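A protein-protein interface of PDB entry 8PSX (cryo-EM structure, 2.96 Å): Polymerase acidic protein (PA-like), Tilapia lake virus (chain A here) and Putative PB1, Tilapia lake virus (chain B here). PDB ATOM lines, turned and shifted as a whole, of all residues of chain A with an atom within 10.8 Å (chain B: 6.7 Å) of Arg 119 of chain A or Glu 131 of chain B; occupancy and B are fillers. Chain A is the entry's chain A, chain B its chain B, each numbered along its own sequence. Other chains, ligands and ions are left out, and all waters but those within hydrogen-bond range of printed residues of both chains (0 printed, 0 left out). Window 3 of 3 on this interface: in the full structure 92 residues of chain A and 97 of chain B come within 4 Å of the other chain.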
ATOM      1  N   SER A 111      15.862   9.898  29.573  1.00  0.00           N
ATOM      2  CA  SER A 111      16.270  11.289  29.730  1.00  0.00           C
ATOM      3  C   SER A 111      15.096  12.255  29.641  1.00  0.00           C
ATOM      4  O   SER A 111      15.194  13.377  30.148  1.00  0.00           O
ATOM      5  CB  SER A 111      17.311  11.650  28.672  1.00  0.00           C
ATOM      6  OG  SER A 111      16.759  11.574  27.369  1.00  0.00           O
ATOM      7  N   TYR A 112      13.996  11.850  29.009  1.00  0.00           N
ATOM      8  CA  TYR A 112      12.810  12.684  28.873  1.00  0.00           C
ATOM      9  C   TYR A 112      11.754  12.370  29.924  1.00  0.00           C
ATOM     10  O   TYR A 112      10.623  12.853  29.817  1.00  0.00           O
ATOM     11  CB  TYR A 112      12.211  12.523  27.474  1.00  0.00           C
ATOM     12  CG  TYR A 112      12.020  11.085  27.052  1.00  0.00           C
ATOM     13  CD1 TYR A 112      10.938  10.346  27.509  1.00  0.00           C
ATOM     14  CD2 TYR A 112      12.925  10.466  26.203  1.00  0.00           C
ATOM     15  CE1 TYR A 112      10.762   9.031  27.130  1.00  0.00           C
ATOM     16  CE2 TYR A 112      12.757   9.152  25.818  1.00  0.00           C
ATOM     17  CZ  TYR A 112      11.675   8.441  26.284  1.00  0.00           C
ATOM     18  OH  TYR A 112      11.505   7.131  25.903  1.00  0.00           O
ATOM     19  N   ASP A 113      12.097  11.568  30.934  1.00  0.00           N
ATOM     20  CA  ASP A 113      11.108  11.147  31.922  1.00  0.00           C
ATOM     21  C   ASP A 113      10.554  12.338  32.696  1.00  0.00           C
ATOM     22  O   ASP A 113       9.337  12.468  32.871  1.00  0.00           O
ATOM     23  CB  ASP A 113      11.737  10.132  32.875  1.00  0.00           C
ATOM     24  CG  ASP A 113      10.778   9.671  33.947  1.00  0.00           C
ATOM     25  OD1 ASP A 113      10.724  10.318  35.012  1.00  0.00           O
ATOM     26  OD2 ASP A 113      10.078   8.664  33.724  1.00  0.00           O
ATOM     27  N   ALA A 114      11.436  13.220  33.169  1.00  0.00           N
ATOM     28  CA  ALA A 114      10.988  14.344  33.987  1.00  0.00           C
ATOM     29  C   ALA A 114      10.145  15.320  33.176  1.00  0.00           C
ATOM     30  O   ALA A 114       9.173  15.886  33.691  1.00  0.00           O
ATOM     31  CB  ALA A 114      12.191  15.056  34.602  1.00  0.00           C
ATOM     32  N   GLU A 115      10.507  15.544  31.911  1.00  0.00           N
ATOM     33  CA  GLU A 115       9.731  16.458  31.080  1.00  0.00           C
ATOM     34  C   GLU A 115       8.312  15.938  30.884  1.00  0.00           C
ATOM     35  O   GLU A 115       7.340  16.691  31.007  1.00  0.00           O
ATOM     36  CB  GLU A 115      10.434  16.664  29.736  1.00  0.00           C
ATOM     37  CG  GLU A 115       9.509  16.698  28.529  1.00  0.00           C
ATOM     38  CD  GLU A 115      10.232  17.084  27.254  1.00  0.00           C
ATOM     39  OE1 GLU A 115      11.458  16.859  27.168  1.00  0.00           O
ATOM     40  OE2 GLU A 115       9.574  17.615  26.336  1.00  0.00           O
ATOM     41  N   LEU A 116       8.173  14.643  30.591  1.00  0.00           N
ATOM     42  CA  LEU A 116       6.843  14.063  30.444  1.00  0.00           C
ATOM     43  C   LEU A 116       6.084  14.084  31.764  1.00  0.00           C
ATOM     44  O   LEU A 116       4.866  14.288  31.780  1.00  0.00           O
ATOM     45  CB  LEU A 116       6.945  12.636  29.906  1.00  0.00           C
ATOM     46  CG  LEU A 116       7.296  12.481  28.424  1.00  0.00           C
ATOM     47  CD1 LEU A 116       7.356  11.012  28.050  1.00  0.00           C
ATOM     48  CD2 LEU A 116       6.301  13.215  27.539  1.00  0.00           C
ATOM     49  N   ARG A 117       6.781  13.863  32.880  1.00  0.00           N
ATOM     50  CA  ARG A 117       6.121  13.929  34.180  1.00  0.00           C
ATOM     51  C   ARG A 117       5.558  15.320  34.441  1.00  0.00           C
ATOM     52  O   ARG A 117       4.427  15.464  34.918  1.00  0.00           O
ATOM     53  CB  ARG A 117       7.100  13.533  35.284  1.00  0.00           C
ATOM     54  CG  ARG A 117       7.048  12.068  35.656  1.00  0.00           C
ATOM     55  CD  ARG A 117       8.063  11.732  36.729  1.00  0.00           C
ATOM     56  NE  ARG A 117       8.339  10.302  36.792  1.00  0.00           N
ATOM     57  CZ  ARG A 117       7.488   9.394  37.249  1.00  0.00           C
ATOM     58  NH1 ARG A 117       6.285   9.731  37.684  1.00  0.00           N
ATOM     59  NH2 ARG A 117       7.852   8.115  37.269  1.00  0.00           N
ATOM     60  N   GLU A 118       6.336  16.359  34.134  1.00  0.00           N
ATOM     61  CA  GLU A 118       5.839  17.721  34.297  1.00  0.00           C
ATOM     62  C   GLU A 118       4.673  17.995  33.353  1.00  0.00           C
ATOM     63  O   GLU A 118       3.683  18.627  33.743  1.00  0.00           O
ATOM     64  CB  GLU A 118       6.967  18.723  34.062  1.00  0.00           C
ATOM     65  CG  GLU A 118       7.618  19.220  35.341  1.00  0.00           C
ATOM     66  CD  GLU A 118       6.804  20.297  36.029  1.00  0.00           C
ATOM     67  OE1 GLU A 118       5.642  20.513  35.626  1.00  0.00           O
ATOM     68  OE2 GLU A 118       7.324  20.927  36.974  1.00  0.00           O
ATOM     69  N   ARG A 119       4.772  17.525  32.106  1.00  0.00           N
ATOM     70  CA  ARG A 119       3.657  17.658  31.174  1.00  0.00           C
ATOM     71  C   ARG A 119       2.388  17.058  31.762  1.00  0.00           C
ATOM     72  O   ARG A 119       1.314  17.666  31.712  1.00  0.00           O
ATOM     73  CB  ARG A 119       3.995  16.975  29.849  1.00  0.00           C
ATOM     74  CG  ARG A 119       4.994  17.712  28.987  1.00  0.00           C
ATOM     75  CD  ARG A 119       4.737  17.442  27.519  1.00  0.00           C
ATOM     76  NE  ARG A 119       5.949  17.566  26.717  1.00  0.00           N
ATOM     77  CZ  ARG A 119       6.105  17.044  25.509  1.00  0.00           C
ATOM     78  NH1 ARG A 119       5.140  16.354  24.923  1.00  0.00           N
ATOM     79  NH2 ARG A 119       7.259  17.218  24.872  1.00  0.00           N
ATOM     80  N   LEU A 120       2.499  15.854  32.322  1.00  0.00           N
ATOM     81  CA  LEU A 120       1.345  15.213  32.940  1.00  0.00           C
ATOM     82  C   LEU A 120       0.822  16.036  34.107  1.00  0.00           C
ATOM     83  O   LEU A 120      -0.392  16.206  34.262  1.00  0.00           O
ATOM     84  CB  LEU A 120       1.720  13.806  33.407  1.00  0.00           C
ATOM     85  CG  LEU A 120       0.630  12.732  33.391  1.00  0.00           C
ATOM     86  CD1 LEU A 120      -0.068  12.659  32.040  1.00  0.00           C
ATOM     87  CD2 LEU A 120       1.223  11.385  33.759  1.00  0.00           C
ATOM     88  N   LEU A 121       1.725  16.556  34.939  1.00  0.00           N
ATOM     89  CA  LEU A 121       1.295  17.341  36.092  1.00  0.00           C
ATOM     90  C   LEU A 121       0.521  18.578  35.655  1.00  0.00           C
ATOM     91  O   LEU A 121      -0.429  18.994  36.328  1.00  0.00           O
ATOM     92  CB  LEU A 121       2.509  17.723  36.944  1.00  0.00           C
ATOM     93  CG  LEU A 121       2.349  18.835  37.986  1.00  0.00           C
ATOM     94  CD1 LEU A 121       3.323  18.608  39.126  1.00  0.00           C
ATOM     95  CD2 LEU A 121       2.585  20.219  37.387  1.00  0.00           C
ATOM     96  N   GLU A 122       0.916  19.185  34.535  1.00  0.00           N
ATOM     97  CA  GLU A 122       0.217  20.364  34.038  1.00  0.00           C
ATOM     98  C   GLU A 122      -1.141  20.039  33.429  1.00  0.00           C
ATOM     99  O   GLU A 122      -1.905  20.967  33.143  1.00  0.00           O
ATOM    100  CB  GLU A 122       1.076  21.084  32.997  1.00  0.00           C
ATOM    101  CG  GLU A 122       2.390  21.628  33.531  1.00  0.00           C
ATOM    102  CD  GLU A 122       2.204  22.541  34.725  1.00  0.00           C
ATOM    103  OE1 GLU A 122       1.196  23.276  34.759  1.00  0.00           O
ATOM    104  OE2 GLU A 122       3.066  22.523  35.628  1.00  0.00           O
ATOM    105  N   LEU A 123      -1.457  18.766  33.217  1.00  0.00           N
ATOM    106  CA  LEU A 123      -2.710  18.384  32.590  1.00  0.00           C
ATOM    107  C   LEU A 123      -3.813  18.224  33.633  1.00  0.00           C
ATOM    108  O   LEU A 123      -3.541  18.143  34.833  1.00  0.00           O
ATOM    109  CB  LEU A 123      -2.524  17.090  31.804  1.00  0.00           C
ATOM    110  CG  LEU A 123      -1.809  17.251  30.459  1.00  0.00           C
ATOM    111  CD1 LEU A 123      -1.390  15.900  29.908  1.00  0.00           C
ATOM    112  CD2 LEU A 123      -2.691  17.984  29.463  1.00  0.00           C
ATOM    113  N   PRO A 124      -5.076  18.181  33.200  1.00  0.00           N
ATOM    114  CA  PRO A 124      -6.180  18.140  34.166  1.00  0.00           C
ATOM    115  C   PRO A 124      -6.135  16.892  35.034  1.00  0.00           C
ATOM    116  O   PRO A 124      -5.642  15.838  34.628  1.00  0.00           O
ATOM    117  CB  PRO A 124      -7.432  18.153  33.280  1.00  0.00           C
ATOM    118  CG  PRO A 124      -6.976  18.616  31.946  1.00  0.00           C
ATOM    119  CD  PRO A 124      -5.561  18.183  31.811  1.00  0.00           C
ATOM    120  N   HIS A 125      -6.657  17.029  36.248  1.00  0.00           N
ATOM    121  CA  HIS A 125      -6.749  15.939  37.202  1.00  0.00           C
ATOM    122  C   HIS A 125      -8.184  15.804  37.686  1.00  0.00           C
ATOM    123  O   HIS A 125      -8.945  16.776  37.658  1.00  0.00           O
ATOM    124  CB  HIS A 125      -5.827  16.169  38.406  1.00  0.00           C
ATOM    125  CG  HIS A 125      -4.381  16.289  38.046  1.00  0.00           C
ATOM    126  ND1 HIS A 125      -3.550  15.195  37.931  1.00  0.00           N
ATOM    127  CD2 HIS A 125      -3.616  17.373  37.779  1.00  0.00           C
ATOM    128  CE1 HIS A 125      -2.336  15.601  37.606  1.00  0.00           C
ATOM    129  NE2 HIS A 125      -2.349  16.917  37.507  1.00  0.00           N
ATOM    130  N   SER B 120      16.536  12.672  23.375  1.00  0.00           N
ATOM    131  CA  SER B 120      15.690  13.817  23.077  1.00  0.00           C
ATOM    132  C   SER B 120      14.410  13.314  22.429  1.00  0.00           C
ATOM    133  O   SER B 120      14.453  12.442  21.558  1.00  0.00           O
ATOM    134  CB  SER B 120      16.400  14.811  22.150  1.00  0.00           C
ATOM    135  OG  SER B 120      15.726  16.057  22.124  1.00  0.00           O
ATOM    136  N   LEU B 121      13.275  13.870  22.856  1.00  0.00           N
ATOM    137  CA  LEU B 121      12.004  13.478  22.263  1.00  0.00           C
ATOM    138  C   LEU B 121      11.949  13.802  20.777  1.00  0.00           C
ATOM    139  O   LEU B 121      11.183  13.170  20.043  1.00  0.00           O
ATOM    140  CB  LEU B 121      10.847  14.164  22.991  1.00  0.00           C
ATOM    141  CG  LEU B 121      10.598  13.701  24.429  1.00  0.00           C
ATOM    142  CD1 LEU B 121       9.664  14.660  25.141  1.00  0.00           C
ATOM    143  CD2 LEU B 121      10.039  12.288  24.459  1.00  0.00           C
ATOM    144  N   SER B 122      12.743  14.769  20.321  1.00  0.00           N
ATOM    145  CA  SER B 122      12.821  15.107  18.907  1.00  0.00           C
ATOM    146  C   SER B 122      13.788  14.220  18.136  1.00  0.00           C
ATOM    147  O   SER B 122      13.757  14.227  16.901  1.00  0.00           O
ATOM    148  CB  SER B 122      13.240  16.571  18.743  1.00  0.00           C
ATOM    149  OG  SER B 122      14.583  16.763  19.147  1.00  0.00           O
ATOM    150  N   GLU B 123      14.638  13.463  18.825  1.00  0.00           N
ATOM    151  CA  GLU B 123      15.590  12.595  18.148  1.00  0.00           C
ATOM    152  C   GLU B 123      14.861  11.587  17.270  1.00  0.00           C
ATOM    153  O   GLU B 123      13.832  11.028  17.660  1.00  0.00           O
ATOM    154  CB  GLU B 123      16.461  11.870  19.174  1.00  0.00           C
ATOM    155  CG  GLU B 123      17.487  10.931  18.567  1.00  0.00           C
ATOM    156  CD  GLU B 123      18.541  10.496  19.564  1.00  0.00           C
ATOM    157  OE1 GLU B 123      18.992  11.345  20.360  1.00  0.00           O
ATOM    158  OE2 GLU B 123      18.923   9.306  19.550  1.00  0.00           O
ATOM    159  N   THR B 128      10.433   8.791  12.359  1.00  0.00           N
ATOM    160  CA  THR B 128       9.581   9.147  13.486  1.00  0.00           C
ATOM    161  C   THR B 128      10.427   9.482  14.707  1.00  0.00           C
ATOM    162  O   THR B 128      11.658   9.416  14.652  1.00  0.00           O
ATOM    163  CB  THR B 128       8.608   8.011  13.815  1.00  0.00           C
ATOM    164  OG1 THR B 128       7.658   8.459  14.788  1.00  0.00           O
ATOM    165  CG2 THR B 128       9.353   6.803  14.360  1.00  0.00           C
ATOM    166  N   SER B 129       9.777   9.843  15.810  1.00  0.00           N
ATOM    167  CA  SER B 129      10.472  10.130  17.055  1.00  0.00           C
ATOM    168  C   SER B 129       9.582   9.705  18.213  1.00  0.00           C
ATOM    169  O   SER B 129       8.434   9.297  18.024  1.00  0.00           O
ATOM    170  CB  SER B 129      10.835  11.613  17.166  1.00  0.00           C
ATOM    171  OG  SER B 129       9.673  12.417  17.252  1.00  0.00           O
ATOM    172  N   VAL B 130      10.129   9.802  19.427  1.00  0.00           N
ATOM    173  CA  VAL B 130       9.344   9.476  20.614  1.00  0.00           C
ATOM    174  C   VAL B 130       8.182  10.449  20.760  1.00  0.00           C
ATOM    175  O   VAL B 130       7.087  10.067  21.186  1.00  0.00           O
ATOM    176  CB  VAL B 130      10.238   9.473  21.867  1.00  0.00           C
ATOM    177  CG1 VAL B 130       9.414   9.160  23.107  1.00  0.00           C
ATOM    178  CG2 VAL B 130      11.360   8.471  21.708  1.00  0.00           C
ATOM    179  N   GLU B 131       8.402  11.719  20.421  1.00  0.00           N
ATOM    180  CA  GLU B 131       7.320  12.695  20.485  1.00  0.00           C
ATOM    181  C   GLU B 131       6.200  12.328  19.520  1.00  0.00           C
ATOM    182  O   GLU B 131       5.019  12.338  19.883  1.00  0.00           O
ATOM    183  CB  GLU B 131       7.860  14.092  20.181  1.00  0.00           C
ATOM    184  CG  GLU B 131       6.878  15.210  20.470  1.00  0.00           C
ATOM    185  CD  GLU B 131       6.759  15.510  21.950  1.00  0.00           C
ATOM    186  OE1 GLU B 131       7.625  16.233  22.484  1.00  0.00           O
ATOM    187  OE2 GLU B 131       5.798  15.020  22.581  1.00  0.00           O
ATOM    188  N   GLU B 132       6.557  11.990  18.279  1.00  0.00           N
ATOM    189  CA  GLU B 132       5.546  11.600  17.304  1.00  0.00           C
ATOM    190  C   GLU B 132       4.861  10.304  17.712  1.00  0.00           C
ATOM    191  O   GLU B 132       3.649  10.148  17.526  1.00  0.00           O
ATOM    192  CB  GLU B 132       6.176  11.459  15.921  1.00  0.00           C
ATOM    193  CG  GLU B 132       5.180  11.579  14.783  1.00  0.00           C
ATOM    194  CD  GLU B 132       5.665  10.917  13.511  1.00  0.00           C
ATOM    195  OE1 GLU B 132       5.561  11.545  12.437  1.00  0.00           O
ATOM    196  OE2 GLU B 132       6.147   9.768  13.583  1.00  0.00           O
ATOM    197  N   LEU B 133       5.622   9.353  18.256  1.00  0.00           N
ATOM    198  CA  LEU B 133       5.019   8.102  18.699  1.00  0.00           C
ATOM    199  C   LEU B 133       4.016   8.343  19.817  1.00  0.00           C
ATOM    200  O   LEU B 133       2.923   7.769  19.814  1.00  0.00           O
ATOM    201  CB  LEU B 133       6.105   7.127  19.155  1.00  0.00           C
ATOM    202  CG  LEU B 133       6.910   6.452  18.044  1.00  0.00           C
ATOM    203  CD1 LEU B 133       8.104   5.716  18.625  1.00  0.00           C
ATOM    204  CD2 LEU B 133       6.038   5.503  17.238  1.00  0.00           C
ATOM    205  N   LEU B 134       4.368   9.192  20.785  1.00  0.00           N
ATOM    206  CA  LEU B 134       3.438   9.505  21.863  1.00  0.00           C
ATOM    207  C   LEU B 134       2.214  10.238  21.335  1.00  0.00           C
ATOM    208  O   LEU B 134       1.095  10.015  21.809  1.00  0.00           O
ATOM    209  CB  LEU B 134       4.137  10.338  22.939  1.00  0.00           C
ATOM    210  CG  LEU B 134       5.169   9.604  23.796  1.00  0.00           C
ATOM    211  CD1 LEU B 134       5.960  10.588  24.638  1.00  0.00           C
ATOM    212  CD2 LEU B 134       4.497   8.569  24.677  1.00  0.00           C
ATOM    213  N   SER B 135       2.406  11.126  20.359  1.00  0.00           N
ATOM    214  CA  SER B 135       1.272  11.829  19.772  1.00  0.00           C
ATOM    215  C   SER B 135       0.321  10.857  19.083  1.00  0.00           C
ATOM    216  O   SER B 135      -0.900  10.947  19.241  1.00  0.00           O
ATOM    217  CB  SER B 135       1.773  12.885  18.787  1.00  0.00           C
ATOM    218  OG  SER B 135       0.759  13.242  17.867  1.00  0.00           O
ATOM    219  N   HIS B 136       0.869   9.913  18.314  1.00  0.00           N
ATOM    220  CA  HIS B 136       0.037   9.000  17.537  1.00  0.00           C
ATOM    221  C   HIS B 136      -0.586   7.902  18.388  1.00  0.00           C
ATOM    222  O   HIS B 136      -1.666   7.407  18.051  1.00  0.00           O
ATOM    223  CB  HIS B 136       0.857   8.370  16.412  1.00  0.00           C
ATOM    224  CG  HIS B 136       1.169   9.313  15.293  1.00  0.00           C
ATOM    225  ND1 HIS B 136       1.646   8.886  14.073  1.00  0.00           N
ATOM    226  CD2 HIS B 136       1.072  10.660  15.208  1.00  0.00           C
ATOM    227  CE1 HIS B 136       1.831   9.930  13.285  1.00  0.00           C
ATOM    228  NE2 HIS B 136       1.490  11.019  13.949  1.00  0.00           N
ATOM    229  N   TYR B 244       0.919   9.162  30.051  1.00  0.00           N
ATOM    230  CA  TYR B 244       0.822  10.377  29.254  1.00  0.00           C
ATOM    231  C   TYR B 244      -0.090  10.171  28.053  1.00  0.00           C
ATOM    232  O   TYR B 244      -0.940  11.018  27.757  1.00  0.00           O
ATOM    233  CB  TYR B 244       2.214  10.813  28.804  1.00  0.00           C
ATOM    234  CG  TYR B 244       2.234  12.087  27.998  1.00  0.00           C
ATOM    235  CD1 TYR B 244       1.982  13.312  28.596  1.00  0.00           C
ATOM    236  CD2 TYR B 244       2.511  12.067  26.640  1.00  0.00           C
ATOM    237  CE1 TYR B 244       2.003  14.479  27.864  1.00  0.00           C
ATOM    238  CE2 TYR B 244       2.533  13.228  25.902  1.00  0.00           C
ATOM    239  CZ  TYR B 244       2.279  14.432  26.518  1.00  0.00           C
ATOM    240  OH  TYR B 244       2.299  15.593  25.782  1.00  0.00           O
ATOM    241  N   ARG B 248      -3.962  11.913  27.393  1.00  0.00           N
ATOM    242  CA  ARG B 248      -4.157  12.718  26.198  1.00  0.00           C
ATOM    243  C   ARG B 248      -4.918  11.968  25.111  1.00  0.00           C
ATOM    244  O   ARG B 248      -4.893  12.380  23.946  1.00  0.00           O
ATOM    245  CB  ARG B 248      -2.804  13.190  25.667  1.00  0.00           C
ATOM    246  CG  ARG B 248      -2.269  14.418  26.371  1.00  0.00           C
ATOM    247  CD  ARG B 248      -0.909  14.807  25.836  1.00  0.00           C
ATOM    248  NE  ARG B 248      -1.010  15.576  24.600  1.00  0.00           N
ATOM    249  CZ  ARG B 248      -0.374  15.292  23.470  1.00  0.00           C
ATOM    250  NH1 ARG B 248       0.435  14.248  23.368  1.00  0.00           N
ATOM    251  NH2 ARG B 248      -0.552  16.077  22.412  1.00  0.00           N
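The guanidinium group (NH2) of Arg 119 of chain A lies within salt-bridge range of the side-chain carboxylate (OE1) of Glu 131 of chain B (2.6 Å).
OH of Tyr 244 of chain B is in hydrogen-bond range of NH1 of Arg 119 of chain A (3.1 Å).
The side-chain carboxylate (OE2) of Glu 115 of chain A is in salt-bridge range of the guanidinium group (NH2) of Arg 119 of chain A, at 2.8 Å.
The backbone carbonyl oxygen of Leu 123 of chain A lies close to a ring nitrogen (NE2) of His 125 of chain A, at 3.2 Å.
O of Leu 121 of chain B lies within hydrogen-bond range of OG of Ser 129 of chain B (3.3 Å).
O of Leu 121 of chain B is in hydrogen-bond range of N of Glu 131 of chain B, 3.2 Å away.
The side-chain hydroxyl (OG) of Ser 129 of chain B lies close to the backbone NH (N) of Glu 131 of chain B (3.5 Å).
OH of Tyr 244 of chain B sits close to NH1 of Arg 248 of chain B (3.3 Å).
Among the printed residues, merely in contact across the chains: Tyr 112 of chain A with Leu 121 of chain B (3.5 Å), Tyr 112 of chain A with Val 130 of chain B (3.97 Å), Glu 115 of chain A with Leu 121 of chain B (3.2 Å), Leu 116 of chain A with Leu 134 of chain B (3.7 Å), Arg 119 of chain A with Leu 121 of chain B (3.5 Å), Leu 120 of chain A with Tyr 244 of chain B (3.7 Å) and Leu 123 of chain A with Arg 248 of chain B (3.9 Å).
Glu 131 of chain B touches just one residue of chain A: Arg 119 (2.6 Å).
Leu 121 of chain B touches just these residues of chain A: Tyr 112 (3.5 Å), Glu 115 (3.2 Å) and Arg 119 (3.5 Å).
No residue of chain A comes within 4 Å of Ser 129 of chain B.
No residue of chain A comes within 4 Å of Ser 135 of chain B.
Of the printed residues of chain A, Arg 248 of chain B touches Leu 123.
Of the printed residues of chain B, Leu 120 of chain A touches Tyr 244.
Printed residues of chain B within 4 Å of Leu 123 of chain A: Arg 248.
Printed residues of chain A within 4 Å of Tyr 244 of chain B: Arg 119 and Leu 120.
Glu 132 of chain B touches none of the printed residues of chain A.
The nearest printed residue of chain B that does not touch Glu 115 of chain A is Glu 131 of chain B (4.5 Å).
Hydrophobic or aromatic side chains of chain A within 4 Å of the printed part of chain B: Tyr 112, Leu 116, Leu 120 and Leu 123.
Among the printed residues, Asp or Glu carboxylates within 4 Å of a Lys or Arg side-chain nitrogen of the other chain: Arg 119 of chain A with Glu 131 of chain B (2.6 Å).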
